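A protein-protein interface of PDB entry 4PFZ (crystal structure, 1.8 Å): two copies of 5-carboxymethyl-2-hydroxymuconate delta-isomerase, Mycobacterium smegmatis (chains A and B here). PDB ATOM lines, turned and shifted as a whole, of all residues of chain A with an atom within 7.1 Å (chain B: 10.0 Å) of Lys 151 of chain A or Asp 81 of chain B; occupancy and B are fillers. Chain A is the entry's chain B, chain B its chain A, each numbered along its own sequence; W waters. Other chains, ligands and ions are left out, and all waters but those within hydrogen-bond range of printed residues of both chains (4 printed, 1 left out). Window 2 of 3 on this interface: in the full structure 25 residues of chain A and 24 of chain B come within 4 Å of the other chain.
Of chain B, only Val 83 (3.4 Å) comes within 4 Å of Asp 152 of chain A.
Of the printed residues of chain B, Gly 153 of chain A touches Gln 154 (3.0 Å).
Printed residues of chain B within 4 Å of Gln 154 of chain A: Val 83, Gln 154 and Trp 155.
Pro 79 of chain B touches none of the printed residues of chain A.
Of chain A, only Lys 151 (3.2 Å) comes within 4 Å of Asp 81 of chain B.
Printed residues of chain A within 4 Å of Gln 154 of chain B: Gly 153 and Gln 154.
Glu 208 of chain B touches none of the printed residues of chain A.
The nearest printed residue of chain A that does not touch Asp 81 of chain B is Arg 157 of chain A (5.9 Å).
The nearest printed residue of chain A that does not touch Gln 154 of chain B is Gln 149 of chain A (6.6 Å).
The side-chain amino group (NZ) of Lys 151 of chain A lies within salt-bridge range of the side-chain carboxylate (OD2) of Asp 81 of chain B.
The backbone NH of Trp 155 of chain B sits at hydrogen-bond distance from the side-chain amide oxygen of Gln 154 of chain A.
The side-chain amide nitrogen (NE2) of Gln 154 of chain B sits at hydrogen-bond distance from the backbone carbonyl oxygen (O) of Gly 153 of chain A, at 3.0 Å.
Of the 10 printed residues of chain A, 5 touch a printed residue of chain B.
Printed residues of chain A that touch a printed residue of chain B: Lys 151, Asp 152, Gly 153, Gln 154 and Arg 157.
Printed residues of chain B that touch a printed residue of chain A: Asp 81, Val 83, Gln 154, Trp 155 and Trp 209.
Among the printed residues, 7 pairs touch across the chains.
Among the printed residues, Asp or Glu carboxylates within 4 Å of a Lys or Arg side-chain nitrogen of the other chain: Lys 151 of chain A with Asp 81 of chain B.
Water W2 lies within hydrogen-bond range of OD1 of Asp 152 of chain A (2.4 Å) and O of Pro 82 of chain B (3.0 Å).
Water W4 bridges OD2 of Asp 81 of chain B (2.7 Å) and NZ of Lys 151 of chain A (3.4 Å).
Water W1 lies within hydrogen-bond range of the backbone carbonyl oxygen (O) of Pro 82 of chain B (2.8 Å), the side-chain carboxylate (OD2) of Asp 152 of chain A (2.8 Å), the backbone NH (N) of Ile 84 of chain B (3.0 Å) and the indole nitrogen (NE1) of Trp 209 of chain B (3.2 Å).
Water W3 lies within hydrogen-bond range of OE1 of Gln 154 of chain A (2.8 Å) and N of Trp 155 of chain B (3.3 Å).
OD1 of Asp 81 of chain B is in salt-bridge range of NH2 of Arg 205 of chain B.
The side-chain carboxylate (OD2) of Asp 152 of chain A is in salt-bridge range of the guanidinium group (NE) of Arg 157 of chain A (2.8 Å).
Gln 154 of chain B touches its own counterpart, Gln 154 of chain A.
Position printed for both chains: 154.
Of the 7 pairs that touch across the chains among the printed residues, 1 has its exchanged pair printed and touching as well.
Among the printed residues, merely in contact across the chains: Asp 152 of chain A with Val 83 of chain B (3.4 Å), Arg 157 of chain A with Trp 209 of chain B (3.5 Å), Gln 154 of chain A with Gln 154 of chain B (3.6 Å) and Gln 154 of chain A with Val 83 of chain B (3.7 Å).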
ATOM      1  N   ARG A 146     -34.695 -14.681 -28.158  1.00  0.00           N
ATOM      2  CA  ARG A 146     -34.135 -15.994 -27.807  1.00  0.00           C
ATOM      3  C   ARG A 146     -32.869 -16.352 -28.589  1.00  0.00           C
ATOM      4  O   ARG A 146     -32.007 -17.057 -28.076  1.00  0.00           O
ATOM      5  CB  ARG A 146     -35.170 -17.108 -28.017  1.00  0.00           C
ATOM      6  CG  ARG A 146     -36.472 -16.950 -27.252  1.00  0.00           C
ATOM      7  CD  ARG A 146     -36.246 -16.698 -25.765  1.00  0.00           C
ATOM      8  NE  ARG A 146     -35.368 -17.686 -25.145  1.00  0.00           N
ATOM      9  CZ  ARG A 146     -35.784 -18.838 -24.629  1.00  0.00           C
ATOM     10  NH1 ARG A 146     -37.072 -19.171 -24.671  1.00  0.00           N
ATOM     11  NH2 ARG A 146     -34.907 -19.666 -24.076  1.00  0.00           N
ATOM     12  N   ASP A 147     -32.765 -15.896 -29.833  1.00  0.00           N
ATOM     13  CA  ASP A 147     -31.579 -16.187 -30.633  1.00  0.00           C
ATOM     14  C   ASP A 147     -30.332 -15.546 -30.017  1.00  0.00           C
ATOM     15  O   ASP A 147     -29.259 -16.165 -29.950  1.00  0.00           O
ATOM     16  CB  ASP A 147     -31.765 -15.706 -32.082  1.00  0.00           C
ATOM     17  CG  ASP A 147     -32.280 -14.264 -32.172  1.00  0.00           C
ATOM     18  OD1 ASP A 147     -32.914 -13.782 -31.203  1.00  0.00           O
ATOM     19  OD2 ASP A 147     -32.067 -13.620 -33.224  1.00  0.00           O
ATOM     20  N   GLN A 148     -30.486 -14.306 -29.568  1.00  0.00           N
ATOM     21  CA  GLN A 148     -29.388 -13.552 -28.964  1.00  0.00           C
ATOM     22  C   GLN A 148     -28.978 -14.153 -27.631  1.00  0.00           C
ATOM     23  O   GLN A 148     -27.803 -14.123 -27.266  1.00  0.00           O
ATOM     24  CB  GLN A 148     -29.780 -12.084 -28.779  1.00  0.00           C
ATOM     25  CG  GLN A 148     -30.119 -11.416 -30.100  1.00  0.00           C
ATOM     26  CD  GLN A 148     -30.545  -9.972 -29.956  1.00  0.00           C
ATOM     27  OE1 GLN A 148     -30.592  -9.426 -28.849  1.00  0.00           O
ATOM     28  NE2 GLN A 148     -30.880  -9.346 -31.084  1.00  0.00           N
ATOM     29  N   GLN A 149     -29.959 -14.685 -26.904  1.00  0.00           N
ATOM     30  CA  GLN A 149     -29.683 -15.395 -25.664  1.00  0.00           C
ATOM     31  C   GLN A 149     -28.706 -16.532 -25.927  1.00  0.00           C
ATOM     32  O   GLN A 149     -27.697 -16.670 -25.243  1.00  0.00           O
ATOM     33  CB  GLN A 149     -30.977 -15.939 -25.051  1.00  0.00           C
ATOM     34  CG  GLN A 149     -31.340 -15.306 -23.734  1.00  0.00           C
ATOM     35  CD  GLN A 149     -32.603 -15.897 -23.129  1.00  0.00           C
ATOM     36  OE1 GLN A 149     -33.693 -15.768 -23.686  1.00  0.00           O
ATOM     37  NE2 GLN A 149     -32.458 -16.549 -21.985  1.00  0.00           N
ATOM     38  N   ARG A 150     -28.993 -17.331 -26.948  1.00  0.00           N
ATOM     39  CA  ARG A 150     -28.172 -18.502 -27.235  1.00  0.00           C
ATOM     40  C   ARG A 150     -26.781 -18.131 -27.758  1.00  0.00           C
ATOM     41  O   ARG A 150     -25.793 -18.796 -27.442  1.00  0.00           O
ATOM     42  CB  ARG A 150     -28.881 -19.411 -28.233  1.00  0.00           C
ATOM     43  CG  ARG A 150     -29.329 -20.735 -27.626  1.00  0.00           C
ATOM     44  CD  ARG A 150     -30.007 -21.631 -28.651  1.00  0.00           C
ATOM     45  NE  ARG A 150     -31.461 -21.496 -28.615  1.00  0.00           N
ATOM     46  CZ  ARG A 150     -32.153 -20.634 -29.353  1.00  0.00           C
ATOM     47  NH1 ARG A 150     -33.474 -20.581 -29.246  1.00  0.00           N
ATOM     48  NH2 ARG A 150     -31.522 -19.822 -30.196  1.00  0.00           N
ATOM     49  N   LYS A 151     -26.713 -17.070 -28.557  1.00  0.00           N
ATOM     50  CA  LYS A 151     -25.454 -16.621 -29.136  1.00  0.00           C
ATOM     51  C   LYS A 151     -24.514 -16.027 -28.084  1.00  0.00           C
ATOM     52  O   LYS A 151     -23.308 -16.274 -28.104  1.00  0.00           O
ATOM     53  CB  LYS A 151     -25.718 -15.582 -30.229  1.00  0.00           C
ATOM     54  CG  LYS A 151     -24.461 -14.906 -30.780  1.00  0.00           C
ATOM     55  CD  LYS A 151     -24.823 -13.843 -31.821  1.00  0.00           C
ATOM     56  CE  LYS A 151     -23.615 -13.014 -32.239  1.00  0.00           C
ATOM     57  NZ  LYS A 151     -22.644 -13.819 -33.047  1.00  0.00           N
ATOM     58  N   ASP A 152     -25.081 -15.230 -27.181  1.00  0.00           N
ATOM     59  CA  ASP A 152     -24.300 -14.431 -26.236  1.00  0.00           C
ATOM     60  C   ASP A 152     -23.873 -15.192 -24.992  1.00  0.00           C
ATOM     61  O   ASP A 152     -22.850 -14.867 -24.386  1.00  0.00           O
ATOM     62  CB  ASP A 152     -25.096 -13.204 -25.796  1.00  0.00           C
ATOM     63  CG  ASP A 152     -25.166 -12.127 -26.857  1.00  0.00           C
ATOM     64  OD1 ASP A 152     -24.753 -12.380 -28.007  1.00  0.00           O
ATOM     65  OD2 ASP A 152     -25.645 -11.019 -26.527  1.00  0.00           O
ATOM     66  N   GLY A 153     -24.668 -16.184 -24.594  1.00  0.00           N
ATOM     67  CA  GLY A 153     -24.479 -16.824 -23.299  1.00  0.00           C
ATOM     68  C   GLY A 153     -25.083 -15.984 -22.180  1.00  0.00           C
ATOM     69  O   GLY A 153     -26.001 -16.425 -21.480  1.00  0.00           O
ATOM     70  N   GLN A 154     -24.567 -14.769 -22.007  1.00  0.00           N
ATOM     71  CA  GLN A 154     -25.187 -13.778 -21.135  1.00  0.00           C
ATOM     72  C   GLN A 154     -26.515 -13.341 -21.757  1.00  0.00           C
ATOM     73  O   GLN A 154     -26.583 -13.091 -22.958  1.00  0.00           O
ATOM     74  CB  GLN A 154     -24.278 -12.565 -20.930  1.00  0.00           C
ATOM     75  CG  GLN A 154     -22.944 -12.906 -20.305  1.00  0.00           C
ATOM     76  CD  GLN A 154     -23.114 -13.664 -19.002  1.00  0.00           C
ATOM     77  OE1 GLN A 154     -23.528 -13.092 -17.998  1.00  0.00           O
ATOM     78  NE2 GLN A 154     -22.784 -14.953 -19.012  1.00  0.00           N
ATOM     79  N   ARG A 157     -28.241  -8.748 -23.342  1.00  0.00           N
ATOM     80  CA  ARG A 157     -28.586  -8.120 -24.631  1.00  0.00           C
ATOM     81  C   ARG A 157     -29.967  -8.570 -25.076  1.00  0.00           C
ATOM     82  O   ARG A 157     -30.824  -7.740 -25.433  1.00  0.00           O
ATOM     83  CB  ARG A 157     -27.567  -8.435 -25.733  1.00  0.00           C
ATOM     84  CG  ARG A 157     -28.027  -7.901 -27.088  1.00  0.00           C
ATOM     85  CD  ARG A 157     -26.919  -7.911 -28.140  1.00  0.00           C
ATOM     86  NE  ARG A 157     -26.548  -9.257 -28.567  1.00  0.00           N
ATOM     87  CZ  ARG A 157     -26.768  -9.747 -29.783  1.00  0.00           C
ATOM     88  NH1 ARG A 157     -26.383 -10.983 -30.080  1.00  0.00           N
ATOM     89  NH2 ARG A 157     -27.374  -9.005 -30.700  1.00  0.00           N
ATOM     90  N   ALA B  62     -20.634  -3.642 -19.493  1.00  0.00           N
ATOM     91  CA  ALA B  62     -19.273  -4.155 -19.522  1.00  0.00           C
ATOM     92  C   ALA B  62     -19.164  -5.291 -20.513  1.00  0.00           C
ATOM     93  O   ALA B  62     -20.161  -5.927 -20.855  1.00  0.00           O
ATOM     94  CB  ALA B  62     -18.839  -4.618 -18.138  1.00  0.00           C
ATOM     95  N   VAL B  63     -17.943  -5.532 -20.975  1.00  0.00           N
ATOM     96  CA  VAL B  63     -17.681  -6.632 -21.870  1.00  0.00           C
ATOM     97  C   VAL B  63     -16.747  -7.620 -21.179  1.00  0.00           C
ATOM     98  O   VAL B  63     -16.019  -7.255 -20.259  1.00  0.00           O
ATOM     99  CB  VAL B  63     -17.078  -6.130 -23.200  1.00  0.00           C
ATOM    100  CG1 VAL B  63     -15.591  -5.884 -23.060  1.00  0.00           C
ATOM    101  CG2 VAL B  63     -17.365  -7.107 -24.320  1.00  0.00           C
ATOM    102  N   GLY B  64     -16.774  -8.869 -21.620  1.00  0.00           N
ATOM    103  CA  GLY B  64     -15.956  -9.901 -21.004  1.00  0.00           C
ATOM    104  C   GLY B  64     -14.553 -10.006 -21.568  1.00  0.00           C
ATOM    105  O   GLY B  64     -13.592  -9.481 -20.991  1.00  0.00           O
ATOM    106  N   LYS B  65     -14.435 -10.698 -22.697  1.00  0.00           N
ATOM    107  CA  LYS B  65     -13.138 -10.938 -23.329  1.00  0.00           C
ATOM    108  C   LYS B  65     -12.867  -9.893 -24.399  1.00  0.00           C
ATOM    109  O   LYS B  65     -13.647  -9.755 -25.351  1.00  0.00           O
ATOM    110  CB  LYS B  65     -13.097 -12.341 -23.936  1.00  0.00           C
ATOM    111  N   ASN B  66     -11.779  -9.140 -24.250  1.00  0.00           N
ATOM    112  CA  ASN B  66     -11.539  -8.062 -25.202  1.00  0.00           C
ATOM    113  C   ASN B  66     -10.097  -7.605 -25.411  1.00  0.00           C
ATOM    114  O   ASN B  66      -9.870  -6.499 -25.901  1.00  0.00           O
ATOM    115  CB  ASN B  66     -12.366  -6.840 -24.811  1.00  0.00           C
ATOM    116  CG  ASN B  66     -12.710  -5.987 -26.005  1.00  0.00           C
ATOM    117  OD1 ASN B  66     -12.845  -6.500 -27.118  1.00  0.00           O
ATOM    118  ND2 ASN B  66     -12.838  -4.687 -25.796  1.00  0.00           N
ATOM    119  N   ALA B  78     -10.324 -14.561 -35.448  1.00  0.00           N
ATOM    120  CA  ALA B  78     -11.232 -13.424 -35.542  1.00  0.00           C
ATOM    121  C   ALA B  78     -12.109 -13.387 -34.305  1.00  0.00           C
ATOM    122  O   ALA B  78     -12.595 -14.431 -33.861  1.00  0.00           O
ATOM    123  CB  ALA B  78     -12.082 -13.513 -36.797  1.00  0.00           C
ATOM    124  N   PRO B  79     -12.338 -12.188 -33.749  1.00  0.00           N
ATOM    125  CA  PRO B  79     -13.064 -12.224 -32.487  1.00  0.00           C
ATOM    126  C   PRO B  79     -14.547 -12.523 -32.714  1.00  0.00           C
ATOM    127  O   PRO B  79     -15.102 -12.175 -33.758  1.00  0.00           O
ATOM    128  CB  PRO B  79     -12.853 -10.809 -31.921  1.00  0.00           C
ATOM    129  CG  PRO B  79     -12.483  -9.940 -33.117  1.00  0.00           C
ATOM    130  CD  PRO B  79     -12.325 -10.835 -34.328  1.00  0.00           C
ATOM    131  N   GLU B  80     -15.164 -13.200 -31.756  1.00  0.00           N
ATOM    132  CA  GLU B  80     -16.611 -13.369 -31.754  1.00  0.00           C
ATOM    133  C   GLU B  80     -17.250 -12.015 -31.413  1.00  0.00           C
ATOM    134  O   GLU B  80     -16.575 -11.141 -30.864  1.00  0.00           O
ATOM    135  CB  GLU B  80     -17.026 -14.448 -30.749  1.00  0.00           C
ATOM    136  CG  GLU B  80     -15.981 -15.547 -30.539  1.00  0.00           C
ATOM    137  CD  GLU B  80     -16.515 -16.734 -29.747  1.00  0.00           C
ATOM    138  OE1 GLU B  80     -17.740 -16.984 -29.794  1.00  0.00           O
ATOM    139  OE2 GLU B  80     -15.710 -17.422 -29.078  1.00  0.00           O
ATOM    140  N   ASP B  81     -18.534 -11.841 -31.738  1.00  0.00           N
ATOM    141  CA  ASP B  81     -19.233 -10.581 -31.482  1.00  0.00           C
ATOM    142  C   ASP B  81     -19.176 -10.225 -30.000  1.00  0.00           C
ATOM    143  O   ASP B  81     -19.049 -11.117 -29.158  1.00  0.00           O
ATOM    144  CB  ASP B  81     -20.690 -10.664 -31.949  1.00  0.00           C
ATOM    145  CG  ASP B  81     -20.832 -10.555 -33.459  1.00  0.00           C
ATOM    146  OD1 ASP B  81     -19.849 -10.179 -34.137  1.00  0.00           O
ATOM    147  OD2 ASP B  81     -21.937 -10.834 -33.969  1.00  0.00           O
ATOM    148  N   PRO B  82     -19.255  -8.920 -29.674  1.00  0.00           N
ATOM    149  CA  PRO B  82     -19.167  -8.550 -28.258  1.00  0.00           C
ATOM    150  C   PRO B  82     -20.228  -9.232 -27.412  1.00  0.00           C
ATOM    151  O   PRO B  82     -21.352  -9.446 -27.880  1.00  0.00           O
ATOM    152  CB  PRO B  82     -19.393  -7.032 -28.271  1.00  0.00           C
ATOM    153  CG  PRO B  82     -18.959  -6.594 -29.646  1.00  0.00           C
ATOM    154  CD  PRO B  82     -19.364  -7.737 -30.552  1.00  0.00           C
ATOM    155  N   VAL B  83     -19.849  -9.591 -26.188  1.00  0.00           N
ATOM    156  CA  VAL B  83     -20.783 -10.082 -25.178  1.00  0.00           C
ATOM    157  C   VAL B  83     -20.891  -9.080 -24.044  1.00  0.00           C
ATOM    158  O   VAL B  83     -20.028  -9.016 -23.166  1.00  0.00           O
ATOM    159  CB  VAL B  83     -20.343 -11.443 -24.605  1.00  0.00           C
ATOM    160  CG1 VAL B  83     -21.328 -11.929 -23.533  1.00  0.00           C
ATOM    161  CG2 VAL B  83     -20.221 -12.459 -25.718  1.00  0.00           C
ATOM    162  N   ILE B  84     -21.953  -8.283 -24.061  1.00  0.00           N
ATOM    163  CA  ILE B  84     -22.123  -7.284 -23.020  1.00  0.00           C
ATOM    164  C   ILE B  84     -23.046  -7.770 -21.917  1.00  0.00           C
ATOM    165  O   ILE B  84     -23.875  -8.669 -22.114  1.00  0.00           O
ATOM    166  CB  ILE B  84     -22.648  -5.958 -23.590  1.00  0.00           C
ATOM    167  CG1 ILE B  84     -23.896  -6.190 -24.455  1.00  0.00           C
ATOM    168  CG2 ILE B  84     -21.565  -5.271 -24.433  1.00  0.00           C
ATOM    169  CD1 ILE B  84     -24.566  -4.891 -24.901  1.00  0.00           C
ATOM    170  N   GLN B 154     -24.970 -16.913 -15.689  1.00  0.00           N
ATOM    171  CA  GLN B 154     -25.094 -15.466 -15.774  1.00  0.00           C
ATOM    172  C   GLN B 154     -24.088 -14.804 -14.839  1.00  0.00           C
ATOM    173  O   GLN B 154     -23.958 -15.198 -13.683  1.00  0.00           O
ATOM    174  CB  GLN B 154     -26.516 -15.025 -15.420  1.00  0.00           C
ATOM    175  CG  GLN B 154     -27.551 -15.585 -16.365  1.00  0.00           C
ATOM    176  CD  GLN B 154     -27.216 -15.267 -17.807  1.00  0.00           C
ATOM    177  OE1 GLN B 154     -27.296 -14.108 -18.232  1.00  0.00           O
ATOM    178  NE2 GLN B 154     -26.821 -16.280 -18.561  1.00  0.00           N
ATOM    179  N   TRP B 155     -23.392 -13.787 -15.331  1.00  0.00           N
ATOM    180  CA  TRP B 155     -22.290 -13.199 -14.572  1.00  0.00           C
ATOM    181  C   TRP B 155     -22.732 -12.079 -13.636  1.00  0.00           C
ATOM    182  O   TRP B 155     -21.945 -11.593 -12.826  1.00  0.00           O
ATOM    183  CB  TRP B 155     -21.227 -12.650 -15.522  1.00  0.00           C
ATOM    184  CG  TRP B 155     -20.640 -13.651 -16.455  1.00  0.00           C
ATOM    185  CD1 TRP B 155     -20.618 -15.008 -16.315  1.00  0.00           C
ATOM    186  CD2 TRP B 155     -19.975 -13.362 -17.681  1.00  0.00           C
ATOM    187  NE1 TRP B 155     -19.967 -15.581 -17.379  1.00  0.00           N
ATOM    188  CE2 TRP B 155     -19.572 -14.588 -18.239  1.00  0.00           C
ATOM    189  CE3 TRP B 155     -19.690 -12.177 -18.372  1.00  0.00           C
ATOM    190  CZ2 TRP B 155     -18.894 -14.667 -19.453  1.00  0.00           C
ATOM    191  CZ3 TRP B 155     -19.014 -12.259 -19.578  1.00  0.00           C
ATOM    192  CH2 TRP B 155     -18.626 -13.493 -20.102  1.00  0.00           C
ATOM    193  N   LEU B 200      -9.866  -6.202 -28.751  1.00  0.00           N
ATOM    194  CA  LEU B 200     -10.487  -6.994 -29.821  1.00  0.00           C
ATOM    195  C   LEU B 200     -11.597  -6.177 -30.484  1.00  0.00           C
ATOM    196  O   LEU B 200     -11.663  -6.068 -31.714  1.00  0.00           O
ATOM    197  CB  LEU B 200     -11.054  -8.306 -29.271  1.00  0.00           C
ATOM    198  CG  LEU B 200     -10.107  -9.233 -28.501  1.00  0.00           C
ATOM    199  CD1 LEU B 200     -10.804 -10.546 -28.170  1.00  0.00           C
ATOM    200  CD2 LEU B 200      -8.837  -9.485 -29.296  1.00  0.00           C
ATOM    201  N   HIS B 201     -12.471  -5.624 -29.643  1.00  0.00           N
ATOM    202  CA  HIS B 201     -13.502  -4.676 -30.058  1.00  0.00           C
ATOM    203  C   HIS B 201     -13.137  -3.287 -29.545  1.00  0.00           C
ATOM    204  O   HIS B 201     -13.096  -3.063 -28.338  1.00  0.00           O
ATOM    205  CB  HIS B 201     -14.869  -5.113 -29.527  1.00  0.00           C
ATOM    206  CG  HIS B 201     -15.199  -6.541 -29.840  1.00  0.00           C
ATOM    207  ND1 HIS B 201     -15.543  -6.962 -31.108  1.00  0.00           N
ATOM    208  CD2 HIS B 201     -15.207  -7.649 -29.061  1.00  0.00           C
ATOM    209  CE1 HIS B 201     -15.760  -8.266 -31.094  1.00  0.00           C
ATOM    210  NE2 HIS B 201     -15.558  -8.708 -29.866  1.00  0.00           N
ATOM    211  N   ARG B 205     -16.473   0.221 -31.684  1.00  0.00           N
ATOM    212  CA  ARG B 205     -17.261  -0.991 -31.870  1.00  0.00           C
ATOM    213  C   ARG B 205     -18.154  -1.260 -30.668  1.00  0.00           C
ATOM    214  O   ARG B 205     -19.257  -1.752 -30.814  1.00  0.00           O
ATOM    215  CB  ARG B 205     -16.361  -2.203 -32.111  1.00  0.00           C
ATOM    216  CG  ARG B 205     -17.127  -3.514 -32.284  1.00  0.00           C
ATOM    217  CD  ARG B 205     -17.659  -3.658 -33.709  1.00  0.00           C
ATOM    218  NE  ARG B 205     -18.677  -4.701 -33.847  1.00  0.00           N
ATOM    219  CZ  ARG B 205     -18.418  -6.003 -33.887  1.00  0.00           C
ATOM    220  NH1 ARG B 205     -17.175  -6.432 -33.773  1.00  0.00           N
ATOM    221  NH2 ARG B 205     -19.405  -6.881 -34.032  1.00  0.00           N
ATOM    222  N   LEU B 206     -17.655  -0.927 -29.483  1.00  0.00           N
ATOM    223  CA  LEU B 206     -18.398  -1.197 -28.257  1.00  0.00           C
ATOM    224  C   LEU B 206     -19.546  -0.203 -28.080  1.00  0.00           C
ATOM    225  O   LEU B 206     -20.628  -0.568 -27.622  1.00  0.00           O
ATOM    226  CB  LEU B 206     -17.463  -1.164 -27.047  1.00  0.00           C
ATOM    227  CG  LEU B 206     -16.427  -2.296 -26.998  1.00  0.00           C
ATOM    228  CD1 LEU B 206     -15.538  -2.138 -25.755  1.00  0.00           C
ATOM    229  CD2 LEU B 206     -17.057  -3.702 -27.039  1.00  0.00           C
ATOM    230  N   GLU B 208     -20.996   1.375 -30.577  1.00  0.00           N
ATOM    231  CA  GLU B 208     -21.927   1.003 -31.625  1.00  0.00           C
ATOM    232  C   GLU B 208     -22.772  -0.192 -31.189  1.00  0.00           C
ATOM    233  O   GLU B 208     -24.001  -0.191 -31.304  1.00  0.00           O
ATOM    234  CB  GLU B 208     -21.172   0.670 -32.902  1.00  0.00           C
ATOM    235  CG  GLU B 208     -22.036   0.288 -34.086  1.00  0.00           C
ATOM    236  CD  GLU B 208     -21.175  -0.070 -35.275  1.00  0.00           C
ATOM    237  OE1 GLU B 208     -20.992   0.790 -36.164  1.00  0.00           O
ATOM    238  OE2 GLU B 208     -20.654  -1.204 -35.293  1.00  0.00           O
ATOM    239  N   TRP B 209     -22.106  -1.221 -30.690  1.00  0.00           N
ATOM    240  CA  TRP B 209     -22.809  -2.447 -30.340  1.00  0.00           C
ATOM    241  C   TRP B 209     -23.819  -2.186 -29.222  1.00  0.00           C
ATOM    242  O   TRP B 209     -24.970  -2.599 -29.321  1.00  0.00           O
ATOM    243  CB  TRP B 209     -21.806  -3.533 -29.949  1.00  0.00           C
ATOM    244  CG  TRP B 209     -22.409  -4.847 -29.604  1.00  0.00           C
ATOM    245  CD1 TRP B 209     -22.794  -5.262 -28.368  1.00  0.00           C
ATOM    246  CD2 TRP B 209     -22.682  -5.936 -30.496  1.00  0.00           C
ATOM    247  NE1 TRP B 209     -23.279  -6.540 -28.430  1.00  0.00           N
ATOM    248  CE2 TRP B 209     -23.236  -6.978 -29.724  1.00  0.00           C
ATOM    249  CE3 TRP B 209     -22.521  -6.129 -31.869  1.00  0.00           C
ATOM    250  CZ2 TRP B 209     -23.619  -8.204 -30.276  1.00  0.00           C
ATOM    251  CZ3 TRP B 209     -22.905  -7.350 -32.422  1.00  0.00           C
ATOM    252  CH2 TRP B 209     -23.454  -8.366 -31.628  1.00  0.00           C
ATOM    253  N   THR B 210     -23.399  -1.457 -28.194  1.00  0.00           N
ATOM    254  CA  THR B 210     -24.236  -1.219 -27.033  1.00  0.00           C
ATOM    255  C   THR B 210     -25.410  -0.284 -27.366  1.00  0.00           C
ATOM    256  O   THR B 210     -26.527  -0.549 -26.972  1.00  0.00           O
ATOM    257  CB  THR B 210     -23.426  -0.619 -25.856  1.00  0.00           C
ATOM    258  OG1 THR B 210     -22.303  -1.459 -25.549  1.00  0.00           O
ATOM    259  CG2 THR B 210     -24.296  -0.491 -24.629  1.00  0.00           C
HETATM  260  O   HOH W   1     -23.686  -8.999 -26.452  1.00  0.00           O
HETATM  261  O   HOH W   2     -22.727 -11.786 -29.241  1.00  0.00           O
HETATM  262  O   HOH W   3     -24.940 -11.131 -16.634  1.00  0.00           O
HETATM  263  O   HOH W   4     -22.184 -12.459 -36.171  1.00  0.00           O
